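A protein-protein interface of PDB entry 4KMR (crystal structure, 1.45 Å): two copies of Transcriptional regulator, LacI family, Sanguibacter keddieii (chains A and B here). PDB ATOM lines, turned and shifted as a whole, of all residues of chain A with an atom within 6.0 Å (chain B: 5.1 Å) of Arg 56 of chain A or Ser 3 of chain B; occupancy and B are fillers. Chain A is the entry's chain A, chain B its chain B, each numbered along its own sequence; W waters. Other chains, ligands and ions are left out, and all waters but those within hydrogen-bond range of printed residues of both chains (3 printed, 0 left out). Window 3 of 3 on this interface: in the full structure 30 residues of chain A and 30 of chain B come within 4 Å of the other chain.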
ATOM      1  N   LEU A  37      37.002 -28.498   9.116  1.00  0.00           N
ATOM      2  CA  LEU A  37      35.998 -29.204   8.276  1.00  0.00           C
ATOM      3  C   LEU A  37      36.366 -28.918   6.817  1.00  0.00           C
ATOM      4  O   LEU A  37      36.383 -27.751   6.406  1.00  0.00           O
ATOM      5  CB  LEU A  37      34.609 -28.684   8.639  1.00  0.00           C
ATOM      6  CG  LEU A  37      33.417 -29.338   8.020  1.00  0.00           C
ATOM      7  CD1 LEU A  37      32.191 -28.772   8.703  1.00  0.00           C
ATOM      8  CD2 LEU A  37      33.365 -29.127   6.515  1.00  0.00           C
ATOM      9  N   GLU A  39      35.518 -29.153   2.917  1.00  0.00           N
ATOM     10  CA  GLU A  39      34.458 -29.292   1.943  1.00  0.00           C
ATOM     11  C   GLU A  39      35.095 -29.171   0.585  1.00  0.00           C
ATOM     12  O   GLU A  39      36.138 -28.496   0.415  1.00  0.00           O
ATOM     13  CB  GLU A  39      33.406 -28.178   2.121  1.00  0.00           C
ATOM     14  CG  GLU A  39      32.520 -28.362   3.335  1.00  0.00           C
ATOM     15  CD  GLU A  39      31.323 -29.268   3.067  1.00  0.00           C
ATOM     16  OE1 GLU A  39      30.416 -28.827   2.323  1.00  0.00           O
ATOM     17  OE2 GLU A  39      31.255 -30.387   3.654  1.00  0.00           O
ATOM     18  N   ASN A  54      24.359 -22.498   3.412  1.00  0.00           N
ATOM     19  CA  ASN A  54      23.614 -23.723   3.771  1.00  0.00           C
ATOM     20  C   ASN A  54      23.902 -24.166   5.215  1.00  0.00           C
ATOM     21  O   ASN A  54      25.022 -24.024   5.679  1.00  0.00           O
ATOM     22  CB  ASN A  54      23.938 -24.832   2.743  1.00  0.00           C
ATOM     23  CG  ASN A  54      23.274 -26.193   3.053  1.00  0.00           C
ATOM     24  OD1 ASN A  54      22.380 -26.309   3.886  1.00  0.00           O
ATOM     25  ND2 ASN A  54      23.751 -27.237   2.374  1.00  0.00           N
ATOM     26  N   PRO A  55      22.875 -24.652   5.940  1.00  0.00           N
ATOM     27  CA  PRO A  55      23.100 -25.144   7.315  1.00  0.00           C
ATOM     28  C   PRO A  55      24.019 -26.386   7.410  1.00  0.00           C
ATOM     29  O   PRO A  55      24.365 -26.850   8.512  1.00  0.00           O
ATOM     30  CB  PRO A  55      21.682 -25.488   7.798  1.00  0.00           C
ATOM     31  CG  PRO A  55      20.841 -25.558   6.551  1.00  0.00           C
ATOM     32  CD  PRO A  55      21.429 -24.511   5.661  1.00  0.00           C
ATOM     33  N   ARG A  56      24.361 -26.955   6.264  1.00  0.00           N
ATOM     34  CA  ARG A  56      25.282 -28.075   6.221  1.00  0.00           C
ATOM     35  C   ARG A  56      26.567 -27.743   6.977  1.00  0.00           C
ATOM     36  O   ARG A  56      27.081 -28.612   7.666  1.00  0.00           O
ATOM     37  CB  ARG A  56      25.566 -28.457   4.787  1.00  0.00           C
ATOM     38  CG  ARG A  56      26.686 -29.453   4.609  1.00  0.00           C
ATOM     39  CD  ARG A  56      26.737 -29.928   3.158  1.00  0.00           C
ATOM     40  NE  ARG A  56      27.973 -30.651   2.958  1.00  0.00           N
ATOM     41  CZ  ARG A  56      28.172 -31.914   3.336  1.00  0.00           C
ATOM     42  NH1 ARG A  56      29.348 -32.438   3.122  1.00  0.00           N
ATOM     43  NH2 ARG A  56      27.210 -32.667   3.914  1.00  0.00           N
ATOM     44  N   LEU A  57      27.061 -26.498   6.878  1.00  0.00           N
ATOM     45  CA  LEU A  57      28.283 -26.083   7.545  1.00  0.00           C
ATOM     46  C   LEU A  57      28.046 -25.266   8.808  1.00  0.00           C
ATOM     47  O   LEU A  57      28.939 -24.540   9.273  1.00  0.00           O
ATOM     48  CB  LEU A  57      29.158 -25.275   6.588  1.00  0.00           C
ATOM     49  CG  LEU A  57      29.577 -25.965   5.310  1.00  0.00           C
ATOM     50  CD1 LEU A  57      30.523 -25.074   4.523  1.00  0.00           C
ATOM     51  CD2 LEU A  57      30.227 -27.306   5.553  1.00  0.00           C
ATOM     52  N   SER A  58      26.897 -25.504   9.451  1.00  0.00           N
ATOM     53  CA  SER A  58      26.561 -24.790  10.685  1.00  0.00           C
ATOM     54  C   SER A  58      27.516 -25.090  11.846  1.00  0.00           C
ATOM     55  O   SER A  58      27.588 -24.308  12.781  1.00  0.00           O
ATOM     56  CB  SER A  58      25.117 -25.058  11.121  1.00  0.00           C
ATOM     57  OG  SER A  58      24.876 -26.423  11.455  1.00  0.00           O
ATOM     58  N   LEU A  59      28.235 -26.206  11.826  1.00  0.00           N
ATOM     59  CA  LEU A  59      29.172 -26.476  12.877  1.00  0.00           C
ATOM     60  C   LEU A  59      30.324 -25.467  12.864  1.00  0.00           C
ATOM     61  O   LEU A  59      30.957 -25.220  13.893  1.00  0.00           O
ATOM     62  CB  LEU A  59      29.763 -27.859  12.662  1.00  0.00           C
ATOM     63  CG  LEU A  59      30.806 -28.346  13.689  1.00  0.00           C
ATOM     64  CD1 LEU A  59      30.292 -28.404  15.132  1.00  0.00           C
ATOM     65  CD2 LEU A  59      31.280 -29.701  13.243  1.00  0.00           C
ATOM     66  N   ARG A  82      28.198 -16.014   8.620  1.00  0.00           N
ATOM     67  CA  ARG A  82      29.406 -16.844   8.521  1.00  0.00           C
ATOM     68  C   ARG A  82      30.672 -15.943   8.147  1.00  0.00           C
ATOM     69  O   ARG A  82      30.855 -15.464   7.027  1.00  0.00           O
ATOM     70  CB  ARG A  82      29.134 -18.065   7.583  1.00  0.00           C
ATOM     71  CG  ARG A  82      30.111 -19.265   7.579  1.00  0.00           C
ATOM     72  CD  ARG A  82      29.529 -20.495   6.809  1.00  0.00           C
ATOM     73  NE  ARG A  82      28.421 -21.171   7.559  1.00  0.00           N
ATOM     74  CZ  ARG A  82      27.425 -21.942   7.070  1.00  0.00           C
ATOM     75  NH1 ARG A  82      27.306 -22.255   5.757  1.00  0.00           N
ATOM     76  NH2 ARG A  82      26.508 -22.414   7.916  1.00  0.00           N
ATOM     77  N   SER B   3      23.371 -31.944   9.273  1.00  0.00           N
ATOM     78  CA  SER B   3      24.393 -32.948   8.811  1.00  0.00           C
ATOM     79  C   SER B   3      25.207 -33.556   9.946  1.00  0.00           C
ATOM     80  O   SER B   3      25.555 -32.886  10.923  1.00  0.00           O
ATOM     81  CB  SER B   3      25.375 -32.354   7.805  1.00  0.00           C
ATOM     82  OG  SER B   3      24.700 -31.673   6.756  1.00  0.00           O
ATOM     83  N   GLY B   4      25.421 -34.865   9.842  1.00  0.00           N
ATOM     84  CA  GLY B   4      26.236 -35.607  10.763  1.00  0.00           C
ATOM     85  C   GLY B   4      27.699 -35.226  10.493  1.00  0.00           C
ATOM     86  O   GLY B   4      28.045 -34.685   9.421  1.00  0.00           O
ATOM     87  N   VAL B   5      28.546 -35.604  11.419  1.00  0.00           N
ATOM     88  CA  VAL B   5      29.959 -35.229  11.378  1.00  0.00           C
ATOM     89  C   VAL B   5      30.850 -36.439  11.596  1.00  0.00           C
ATOM     90  O   VAL B   5      30.646 -37.193  12.533  1.00  0.00           O
ATOM     91  CB  VAL B   5      30.273 -34.252  12.529  1.00  0.00           C
ATOM     92  CG1 VAL B   5      31.719 -33.756  12.418  1.00  0.00           C
ATOM     93  CG2 VAL B   5      29.289 -33.066  12.549  1.00  0.00           C
ATOM     94  N   ALA B  29      30.941 -39.020   1.814  1.00  0.00           N
ATOM     95  CA  ALA B  29      30.315 -38.482   2.992  1.00  0.00           C
ATOM     96  C   ALA B  29      29.254 -37.424   2.578  1.00  0.00           C
ATOM     97  O   ALA B  29      28.168 -37.418   3.138  1.00  0.00           O
ATOM     98  CB  ALA B  29      31.398 -37.866   3.909  1.00  0.00           C
ATOM     99  N   ALA B  30      29.561 -36.570   1.593  1.00  0.00           N
ATOM    100  CA  ALA B  30      28.616 -35.532   1.186  1.00  0.00           C
ATOM    101  C   ALA B  30      27.332 -36.165   0.625  1.00  0.00           C
ATOM    102  O   ALA B  30      26.210 -35.696   0.888  1.00  0.00           O
ATOM    103  CB  ALA B  30      29.274 -34.602   0.167  1.00  0.00           C
ATOM    104  N   ASP B  33      25.055 -37.000   3.544  1.00  0.00           N
ATOM    105  CA  ASP B  33      24.733 -35.868   4.454  1.00  0.00           C
ATOM    106  C   ASP B  33      25.660 -35.847   5.655  1.00  0.00           C
ATOM    107  O   ASP B  33      25.222 -35.635   6.814  1.00  0.00           O
ATOM    108  CB  ASP B  33      23.240 -35.894   4.894  1.00  0.00           C
ATOM    109  CG  ASP B  33      22.326 -35.651   3.749  1.00  0.00           C
ATOM    110  OD1 ASP B  33      21.144 -36.034   3.816  1.00  0.00           O
ATOM    111  OD2 ASP B  33      22.818 -35.077   2.753  1.00  0.00           O
ATOM    112  N   LEU B  34      26.937 -36.073   5.386  1.00  0.00           N
ATOM    113  CA  LEU B  34      27.945 -35.999   6.419  1.00  0.00           C
ATOM    114  C   LEU B  34      29.016 -34.972   6.020  1.00  0.00           C
ATOM    115  O   LEU B  34      29.325 -34.802   4.814  1.00  0.00           O
ATOM    116  CB  LEU B  34      28.638 -37.330   6.574  1.00  0.00           C
ATOM    117  CG  LEU B  34      27.807 -38.505   7.037  1.00  0.00           C
ATOM    118  CD1 LEU B  34      28.574 -39.823   6.922  1.00  0.00           C
ATOM    119  CD2 LEU B  34      27.275 -38.300   8.462  1.00  0.00           C
ATOM    120  N   VAL B  35      29.534 -34.265   7.026  1.00  0.00           N
ATOM    121  CA  VAL B  35      30.702 -33.392   6.833  1.00  0.00           C
ATOM    122  C   VAL B  35      31.911 -34.106   7.481  1.00  0.00           C
ATOM    123  O   VAL B  35      31.730 -34.931   8.383  1.00  0.00           O
ATOM    124  CB  VAL B  35      30.507 -31.978   7.415  1.00  0.00           C
ATOM    125  CG1 VAL B  35      29.426 -31.238   6.615  1.00  0.00           C
ATOM    126  CG2 VAL B  35      30.179 -32.030   8.907  1.00  0.00           C
HETATM  127  O   HOH W   1      24.603 -29.307   9.826  1.00  0.00           O
HETATM  128  O   HOH W   2      31.685 -34.160   2.879  1.00  0.00           O
HETATM  129  O   HOH W   3      25.668 -32.993   0.927  1.00  0.00           O
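Of the 9 printed residues of chain A, 4 touch a printed residue of chain B.
Of the 8 printed residues of chain B, 6 touch a printed residue of chain A.
Among the printed residues, 8 pairs touch across the chains.
OE2 of Glu 39 of chain A lies within salt-bridge range of NH1 of Arg 56 of chain A (2.9 Å).
The side-chain amide oxygen (OD1) of Asn 54 of chain A lies close to the backbone NH (N) of Arg 56 of chain A.
The backbone NH (N) of Gly 4 of chain B is in hydrogen-bond range of the backbone carbonyl oxygen (O) of Asp 33 of chain B (3.1 Å).
The backbone carbonyl oxygen of Gly 4 of chain B sits at hydrogen-bond distance from the backbone NH of Val 35 of chain B (2.9 Å).
The backbone carbonyl oxygen (O) of Ala 29 of chain B is in hydrogen-bond range of the backbone NH (N) of Leu 34 of chain B (2.9 Å).
Water W3 bridges O of Ala 30 of chain B (2.8 Å) and NH2 of Arg 56 of chain A (3.4 Å).
Water W1 lies within hydrogen-bond range of O of Pro 55 of chain A (2.8 Å), N of Ser 3 of chain B (3.0 Å), OG of Ser 58 of chain A (3.3 Å) and O of Arg 56 of chain A (3.4 Å).
Water W2 lies within hydrogen-bond range of NH1 of Arg 56 of chain A (2.9 Å), O of Leu 34 of chain B (3.1 Å) and N of Ala 30 of chain B (3.5 Å).
No position is printed for both chains.
The guanidinium group of Arg 56 of chain A lies within hydrogen-bond range of the backbone carbonyl oxygen of Leu 34 of chain B.
Arg 56 of chain A touches five residues of chain B.
Ser 3 of chain B touches just one residue of chain A: Arg 56 (3.7 Å).
Printed residues of chain A within 4 Å of Val 35 of chain B: Leu 37, Glu 39 and Arg 56.
Printed residues of chain A within 4 Å of Ala 30 of chain B: Arg 56.
Of the printed residues of chain B, Leu 37 of chain A touches Val 35.
Of the printed residues of chain A, Val 5 of chain B touches Leu 59.
Of the printed residues of chain A, Asp 33 of chain B touches Arg 56.
Asn 54 of chain A touches none of the printed residues of chain B.
Ser 58 of chain A touches none of the printed residues of chain B.
Among the printed residues, pairs that only touch across the chains: Arg 56 of chain A with Val 35 of chain B (3.6 Å), Glu 39 of chain A with Val 35 of chain B (3.6 Å), Arg 56 of chain A with Ala 30 of chain B (3.7 Å), Arg 56 of chain A with Ser 3 of chain B (3.7 Å), Leu 37 of chain A with Val 35 of chain B (3.8 Å), Arg 56 of chain A with Asp 33 of chain B (3.9 Å) and Leu 59 of chain A with Val 5 of chain B (3.97 Å).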
